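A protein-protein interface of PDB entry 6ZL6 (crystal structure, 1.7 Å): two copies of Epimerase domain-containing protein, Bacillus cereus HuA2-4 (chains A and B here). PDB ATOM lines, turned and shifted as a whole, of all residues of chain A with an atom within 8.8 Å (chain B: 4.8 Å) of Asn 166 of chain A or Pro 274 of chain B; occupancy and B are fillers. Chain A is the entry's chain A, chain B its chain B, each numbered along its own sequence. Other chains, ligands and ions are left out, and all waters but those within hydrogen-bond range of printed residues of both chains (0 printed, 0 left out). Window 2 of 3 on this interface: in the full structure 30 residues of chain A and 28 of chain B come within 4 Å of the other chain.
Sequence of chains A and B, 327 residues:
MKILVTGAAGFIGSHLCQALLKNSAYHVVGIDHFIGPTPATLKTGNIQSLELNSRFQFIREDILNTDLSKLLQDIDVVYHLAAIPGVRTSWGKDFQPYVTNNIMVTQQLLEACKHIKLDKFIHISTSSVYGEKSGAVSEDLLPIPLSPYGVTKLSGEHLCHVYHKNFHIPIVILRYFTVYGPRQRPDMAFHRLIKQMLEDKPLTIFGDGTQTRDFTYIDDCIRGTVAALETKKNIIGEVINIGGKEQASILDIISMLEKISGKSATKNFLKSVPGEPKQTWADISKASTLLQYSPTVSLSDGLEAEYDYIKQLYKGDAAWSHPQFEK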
ATOM      1  N   LYS A 114      25.843   7.494   2.315  1.00  0.00           N
ATOM      2  CA  LYS A 114      24.841   6.731   1.516  1.00  0.00           C
ATOM      3  C   LYS A 114      23.428   7.314   1.638  1.00  0.00           C
ATOM      4  O   LYS A 114      22.730   7.341   0.605  1.00  0.00           O
ATOM      5  CB  LYS A 114      24.764   5.269   1.951  1.00  0.00           C
ATOM      6  CG  LYS A 114      25.760   4.367   1.249  1.00  0.00           C
ATOM      7  CD  LYS A 114      26.004   3.043   1.985  1.00  0.00           C
ATOM      8  CE  LYS A 114      24.785   2.426   2.613  1.00  0.00           C
ATOM      9  NZ  LYS A 114      24.829   0.960   2.434  1.00  0.00           N
ATOM     10  N   HIS A 158      38.967   3.821  -6.321  1.00  0.00           N
ATOM     11  CA  HIS A 158      38.156   2.634  -6.702  1.00  0.00           C
ATOM     12  C   HIS A 158      36.971   2.522  -5.752  1.00  0.00           C
ATOM     13  O   HIS A 158      35.834   2.260  -6.267  1.00  0.00           O
ATOM     14  CB  HIS A 158      39.010   1.369  -6.760  1.00  0.00           C
ATOM     15  CG  HIS A 158      39.955   1.310  -7.910  1.00  0.00           C
ATOM     16  ND1 HIS A 158      41.103   0.555  -7.843  1.00  0.00           N
ATOM     17  CD2 HIS A 158      39.969   1.923  -9.111  1.00  0.00           C
ATOM     18  CE1 HIS A 158      41.741   0.646  -9.002  1.00  0.00           C
ATOM     19  NE2 HIS A 158      41.081   1.488  -9.775  1.00  0.00           N
ATOM     20  N   LEU A 159      37.155   2.784  -4.453  1.00  0.00           N
ATOM     21  CA  LEU A 159      36.010   2.780  -3.512  1.00  0.00           C
ATOM     22  C   LEU A 159      35.024   3.867  -3.968  1.00  0.00           C
ATOM     23  O   LEU A 159      33.824   3.591  -3.928  1.00  0.00           O
ATOM     24  CB  LEU A 159      36.464   3.021  -2.082  1.00  0.00           C
ATOM     25  CG  LEU A 159      37.160   1.847  -1.409  1.00  0.00           C
ATOM     26  CD1 LEU A 159      37.901   2.300  -0.180  1.00  0.00           C
ATOM     27  CD2 LEU A 159      36.189   0.737  -1.059  1.00  0.00           C
ATOM     28  N   CYS A 160      35.502   5.039  -4.392  1.00  0.00           N
ATOM     29  CA  CYS A 160      34.598   6.136  -4.869  1.00  0.00           C
ATOM     30  C   CYS A 160      33.708   5.627  -6.019  1.00  0.00           C
ATOM     31  O   CYS A 160      32.461   5.787  -5.943  1.00  0.00           O
ATOM     32  CB  CYS A 160      35.384   7.358  -5.306  1.00  0.00           C
ATOM     33  SG  CYS A 160      36.013   8.311  -3.915  1.00  0.00           S
ATOM     34  N   HIS A 161      34.305   5.020  -7.045  1.00  0.00           N
ATOM     35  CA  HIS A 161      33.578   4.394  -8.180  1.00  0.00           C
ATOM     36  C   HIS A 161      32.558   3.357  -7.664  1.00  0.00           C
ATOM     37  O   HIS A 161      31.385   3.455  -8.094  1.00  0.00           O
ATOM     38  CB  HIS A 161      34.529   3.802  -9.206  1.00  0.00           C
ATOM     39  CG  HIS A 161      35.343   4.834  -9.901  1.00  0.00           C
ATOM     40  ND1 HIS A 161      34.762   5.857 -10.619  1.00  0.00           N
ATOM     41  CD2 HIS A 161      36.685   4.999 -10.023  1.00  0.00           C
ATOM     42  CE1 HIS A 161      35.704   6.639 -11.126  1.00  0.00           C
ATOM     43  NE2 HIS A 161      36.902   6.118 -10.783  1.00  0.00           N
ATOM     44  N   VAL A 162      32.933   2.490  -6.711  1.00  0.00           N
ATOM     45  CA  VAL A 162      32.026   1.462  -6.119  1.00  0.00           C
ATOM     46  C   VAL A 162      30.793   2.146  -5.516  1.00  0.00           C
ATOM     47  O   VAL A 162      29.629   1.713  -5.807  1.00  0.00           O
ATOM     48  CB  VAL A 162      32.755   0.597  -5.077  1.00  0.00           C
ATOM     49  CG1 VAL A 162      31.814  -0.219  -4.218  1.00  0.00           C
ATOM     50  CG2 VAL A 162      33.793  -0.297  -5.732  1.00  0.00           C
ATOM     51  N   TYR A 163      30.997   3.146  -4.667  1.00  0.00           N
ATOM     52  CA  TYR A 163      29.875   3.808  -3.949  1.00  0.00           C
ATOM     53  C   TYR A 163      29.050   4.686  -4.917  1.00  0.00           C
ATOM     54  O   TYR A 163      27.807   4.787  -4.701  1.00  0.00           O
ATOM     55  CB  TYR A 163      30.396   4.486  -2.688  1.00  0.00           C
ATOM     56  CG  TYR A 163      30.643   3.502  -1.570  1.00  0.00           C
ATOM     57  CD1 TYR A 163      31.819   2.746  -1.524  1.00  0.00           C
ATOM     58  CD2 TYR A 163      29.722   3.291  -0.568  1.00  0.00           C
ATOM     59  CE1 TYR A 163      32.038   1.819  -0.531  1.00  0.00           C
ATOM     60  CE2 TYR A 163      29.931   2.376   0.446  1.00  0.00           C
ATOM     61  CZ  TYR A 163      31.095   1.618   0.456  1.00  0.00           C
ATOM     62  OH  TYR A 163      31.372   0.706   1.434  1.00  0.00           O
ATOM     63  N   HIS A 164      29.689   5.305  -5.917  1.00  0.00           N
ATOM     64  CA  HIS A 164      28.987   6.019  -7.009  1.00  0.00           C
ATOM     65  C   HIS A 164      28.023   5.024  -7.670  1.00  0.00           C
ATOM     66  O   HIS A 164      26.817   5.266  -7.649  1.00  0.00           O
ATOM     67  CB  HIS A 164      29.970   6.656  -7.988  1.00  0.00           C
ATOM     68  CG  HIS A 164      29.343   7.211  -9.222  1.00  0.00           C
ATOM     69  ND1 HIS A 164      28.225   8.005  -9.192  1.00  0.00           N
ATOM     70  CD2 HIS A 164      29.690   7.115 -10.519  1.00  0.00           C
ATOM     71  CE1 HIS A 164      27.902   8.371 -10.427  1.00  0.00           C
ATOM     72  NE2 HIS A 164      28.769   7.852 -11.249  1.00  0.00           N
ATOM     73  N   LYS A 165      28.526   3.926  -8.216  1.00  0.00           N
ATOM     74  CA  LYS A 165      27.709   3.099  -9.132  1.00  0.00           C
ATOM     75  C   LYS A 165      26.620   2.384  -8.352  1.00  0.00           C
ATOM     76  O   LYS A 165      25.538   2.267  -8.913  1.00  0.00           O
ATOM     77  CB  LYS A 165      28.566   2.166  -9.987  1.00  0.00           C
ATOM     78  CG  LYS A 165      29.120   2.848 -11.228  1.00  0.00           C
ATOM     79  CD  LYS A 165      29.890   1.936 -12.163  1.00  0.00           C
ATOM     80  CE  LYS A 165      31.339   1.732 -11.753  1.00  0.00           C
ATOM     81  NZ  LYS A 165      32.157   2.957 -11.940  1.00  0.00           N
ATOM     82  N   ASN A 166      26.872   2.001  -7.103  1.00  0.00           N
ATOM     83  CA  ASN A 166      25.947   1.177  -6.296  1.00  0.00           C
ATOM     84  C   ASN A 166      24.971   2.065  -5.537  1.00  0.00           C
ATOM     85  O   ASN A 166      23.801   1.656  -5.423  1.00  0.00           O
ATOM     86  CB  ASN A 166      26.692   0.200  -5.403  1.00  0.00           C
ATOM     87  CG  ASN A 166      27.345  -0.873  -6.253  1.00  0.00           C
ATOM     88  OD1 ASN A 166      26.662  -1.758  -6.760  1.00  0.00           O
ATOM     89  ND2 ASN A 166      28.655  -0.785  -6.457  1.00  0.00           N
ATOM     90  N   PHE A 167      25.410   3.205  -5.011  1.00  0.00           N
ATOM     91  CA  PHE A 167      24.618   3.990  -4.030  1.00  0.00           C
ATOM     92  C   PHE A 167      24.422   5.428  -4.507  1.00  0.00           C
ATOM     93  O   PHE A 167      23.835   6.192  -3.732  1.00  0.00           O
ATOM     94  CB  PHE A 167      25.229   3.917  -2.626  1.00  0.00           C
ATOM     95  CG  PHE A 167      25.326   2.510  -2.092  1.00  0.00           C
ATOM     96  CD1 PHE A 167      24.182   1.751  -1.908  1.00  0.00           C
ATOM     97  CD2 PHE A 167      26.552   1.914  -1.834  1.00  0.00           C
ATOM     98  CE1 PHE A 167      24.249   0.440  -1.459  1.00  0.00           C
ATOM     99  CE2 PHE A 167      26.617   0.601  -1.391  1.00  0.00           C
ATOM    100  CZ  PHE A 167      25.471  -0.135  -1.208  1.00  0.00           C
ATOM    101  N   HIS A 168      24.864   5.759  -5.714  1.00  0.00           N
ATOM    102  CA  HIS A 168      24.671   7.078  -6.373  1.00  0.00           C
ATOM    103  C   HIS A 168      25.290   8.202  -5.537  1.00  0.00           C
ATOM    104  O   HIS A 168      24.795   9.323  -5.629  1.00  0.00           O
ATOM    105  CB  HIS A 168      23.178   7.298  -6.678  1.00  0.00           C
ATOM    106  CG  HIS A 168      22.583   6.161  -7.437  1.00  0.00           C
ATOM    107  ND1 HIS A 168      23.055   5.783  -8.683  1.00  0.00           N
ATOM    108  CD2 HIS A 168      21.599   5.291  -7.116  1.00  0.00           C
ATOM    109  CE1 HIS A 168      22.364   4.744  -9.110  1.00  0.00           C
ATOM    110  NE2 HIS A 168      21.470   4.418  -8.163  1.00  0.00           N
ATOM    111  N   ILE A 169      26.369   7.930  -4.796  1.00  0.00           N
ATOM    112  CA  ILE A 169      27.154   9.005  -4.124  1.00  0.00           C
ATOM    113  C   ILE A 169      27.780   9.815  -5.256  1.00  0.00           C
ATOM    114  O   ILE A 169      28.389   9.225  -6.152  1.00  0.00           O
ATOM    115  CB  ILE A 169      28.175   8.440  -3.118  1.00  0.00           C
ATOM    116  CG1 ILE A 169      27.459   7.639  -2.023  1.00  0.00           C
ATOM    117  CG2 ILE A 169      29.034   9.550  -2.529  1.00  0.00           C
ATOM    118  CD1 ILE A 169      28.371   7.112  -0.929  1.00  0.00           C
ATOM    119  N   TRP B  91      30.588  -5.130   2.481  1.00  0.00           N
ATOM    120  CA  TRP B  91      30.044  -3.763   2.741  1.00  0.00           C
ATOM    121  C   TRP B  91      30.173  -3.381   4.213  1.00  0.00           C
ATOM    122  O   TRP B  91      30.341  -4.265   5.064  1.00  0.00           O
ATOM    123  CB  TRP B  91      28.584  -3.606   2.265  1.00  0.00           C
ATOM    124  CG  TRP B  91      28.450  -3.833   0.799  1.00  0.00           C
ATOM    125  CD1 TRP B  91      28.036  -4.989   0.198  1.00  0.00           C
ATOM    126  CD2 TRP B  91      28.795  -2.920  -0.266  1.00  0.00           C
ATOM    127  NE1 TRP B  91      28.099  -4.853  -1.166  1.00  0.00           N
ATOM    128  CE2 TRP B  91      28.534  -3.589  -1.482  1.00  0.00           C
ATOM    129  CE3 TRP B  91      29.278  -1.608  -0.321  1.00  0.00           C
ATOM    130  CZ2 TRP B  91      28.724  -2.987  -2.725  1.00  0.00           C
ATOM    131  CZ3 TRP B  91      29.473  -1.020  -1.550  1.00  0.00           C
ATOM    132  CH2 TRP B  91      29.182  -1.693  -2.736  1.00  0.00           C
ATOM    133  N   LEU B 146      33.516  -3.250  -9.144  1.00  0.00           N
ATOM    134  CA  LEU B 146      32.126  -2.896  -8.769  1.00  0.00           C
ATOM    135  C   LEU B 146      31.899  -3.176  -7.292  1.00  0.00           C
ATOM    136  O   LEU B 146      30.899  -2.683  -6.781  1.00  0.00           O
ATOM    137  CB  LEU B 146      31.152  -3.670  -9.666  1.00  0.00           C
ATOM    138  CG  LEU B 146      30.959  -2.998 -11.026  1.00  0.00           C
ATOM    139  CD1 LEU B 146      30.381  -3.963 -12.040  1.00  0.00           C
ATOM    140  CD2 LEU B 146      30.077  -1.756 -10.890  1.00  0.00           C
ATOM    141  N   SER B 272      18.468  -8.326  -6.488  1.00  0.00           N
ATOM    142  CA  SER B 272      19.880  -8.279  -6.953  1.00  0.00           C
ATOM    143  C   SER B 272      20.781  -7.818  -5.792  1.00  0.00           C
ATOM    144  O   SER B 272      20.309  -7.059  -4.935  1.00  0.00           O
ATOM    145  CB  SER B 272      20.025  -7.379  -8.157  1.00  0.00           C
ATOM    146  OG  SER B 272      19.538  -6.079  -7.864  1.00  0.00           O
ATOM    147  N   VAL B 273      22.033  -8.266  -5.770  1.00  0.00           N
ATOM    148  CA  VAL B 273      23.032  -7.901  -4.722  1.00  0.00           C
ATOM    149  C   VAL B 273      23.866  -6.737  -5.256  1.00  0.00           C
ATOM    150  O   VAL B 273      24.488  -6.854  -6.298  1.00  0.00           O
ATOM    151  CB  VAL B 273      23.920  -9.118  -4.405  1.00  0.00           C
ATOM    152  CG1 VAL B 273      25.187  -8.722  -3.668  1.00  0.00           C
ATOM    153  CG2 VAL B 273      23.155 -10.192  -3.642  1.00  0.00           C
ATOM    154  N   PRO B 274      23.977  -5.596  -4.551  1.00  0.00           N
ATOM    155  CA  PRO B 274      24.890  -4.540  -4.988  1.00  0.00           C
ATOM    156  C   PRO B 274      26.324  -5.087  -5.023  1.00  0.00           C
ATOM    157  O   PRO B 274      26.682  -5.843  -4.123  1.00  0.00           O
ATOM    158  CB  PRO B 274      24.755  -3.461  -3.905  1.00  0.00           C
ATOM    159  CG  PRO B 274      23.409  -3.763  -3.278  1.00  0.00           C
ATOM    160  CD  PRO B 274      23.318  -5.270  -3.282  1.00  0.00           C
ATOM    161  N   GLY B 275      27.089  -4.635  -6.007  1.00  0.00           N
ATOM    162  CA  GLY B 275      28.521  -4.934  -6.142  1.00  0.00           C
ATOM    163  C   GLY B 275      28.770  -6.083  -7.091  1.00  0.00           C
ATOM    164  O   GLY B 275      29.921  -6.285  -7.402  1.00  0.00           O
ATOM    165  N   GLU B 276      27.737  -6.782  -7.582  1.00  0.00           N
ATOM    166  CA  GLU B 276      27.953  -7.927  -8.511  1.00  0.00           C
ATOM    167  C   GLU B 276      27.890  -7.439  -9.953  1.00  0.00           C
ATOM    168  O   GLU B 276      27.025  -6.647 -10.337  1.00  0.00           O
ATOM    169  CB  GLU B 276      26.931  -9.051  -8.288  1.00  0.00           C
ATOM    170  CG  GLU B 276      26.908  -9.596  -6.885  1.00  0.00           C
ATOM    171  CD  GLU B 276      26.258 -10.969  -6.769  1.00  0.00           C
ATOM    172  OE1 GLU B 276      25.083 -11.112  -7.173  1.00  0.00           O
ATOM    173  OE2 GLU B 276      26.918 -11.883  -6.259  1.00  0.00           O
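ND2 of Asn 166 of chain A lies within hydrogen-bond range of O of Leu 146 of chain B, at 3.0 Å. OD1 of Asn 166 of chain A lies within hydrogen-bond range of N of Gly 275 of chain B (3.0 Å).
The backbone carbonyl oxygen of Val 162 of chain A sits at hydrogen-bond distance from the side-chain amide nitrogen of Asn 166 of chain A (2.8 Å). O of Tyr 163 of chain A lies within hydrogen-bond range of N of His 168 of chain A (3.3 Å). The backbone carbonyl oxygen of Tyr 163 of chain A sits at hydrogen-bond distance from the backbone NH of Ile 169 of chain A (3.5 Å). NE1 of Trp 91 of chain B sits at hydrogen-bond distance from O of Pro 274 of chain B (3.4 Å).
CH2 of Trp 91 of chain B touches CG1 of Val 162 of chain A, 3.4 Å away. Val 162 of chain A touches Leu 146 of chain B (CG1 to O, 3.7 Å). OH of Tyr 163 of chain A touches CE3 of Trp 91 of chain B, 3.6 Å away. Leu 146 of chain B touches Lys 165 of chain A. Asn 166 of chain A touches Trp 91 of chain B. CA of Pro 274 of chain B touches OD1 of Asn 166 of chain A (3.7 Å). Phe 167 of chain A touches Trp 91 of chain B (CE2 to CZ3, 3.3 Å).
Of chain B, only Trp 91 (3.9 Å), Leu 146 (3.0 Å), Pro 274 (3.7 Å) and Gly 275 (3.0 Å) come within 4 Å of Asn 166 of chain A. Of chain A, only Asn 166 (3.7 Å) comes within 4 Å of Pro 274 of chain B. Gly 275 of chain B touches just one residue of chain A: Asn 166. Of the printed residues of chain B, Phe 167 of chain A touches Trp 91. Printed residues of chain B within 4 Å of Val 162 of chain A: Trp 91 and Leu 146. His 164 of chain A touches none of the printed residues of chain B. His 161 of chain A touches none of the printed residues of chain B. The nearest printed residue of chain B that does not touch Lys 165 of chain A is Trp 91 of chain B (7.4 Å).
Along chain A the printed residues that touch a printed residue of chain B span positions 162 to 167. Printed residues of chain B that touch a printed residue of chain A: Trp 91, Leu 146, Pro 274 and Gly 275. Hydrophobic or aromatic side chains of chain B within 4 Å of the printed part of chain A: Trp 91, Leu 146 and Pro 274. Among the printed residues, 9 pairs touch across the chains.
No position is printed for both chains. Of the 9 pairs that touch across the chains among the printed residues, none has its exchanged pair printed and touching as well.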
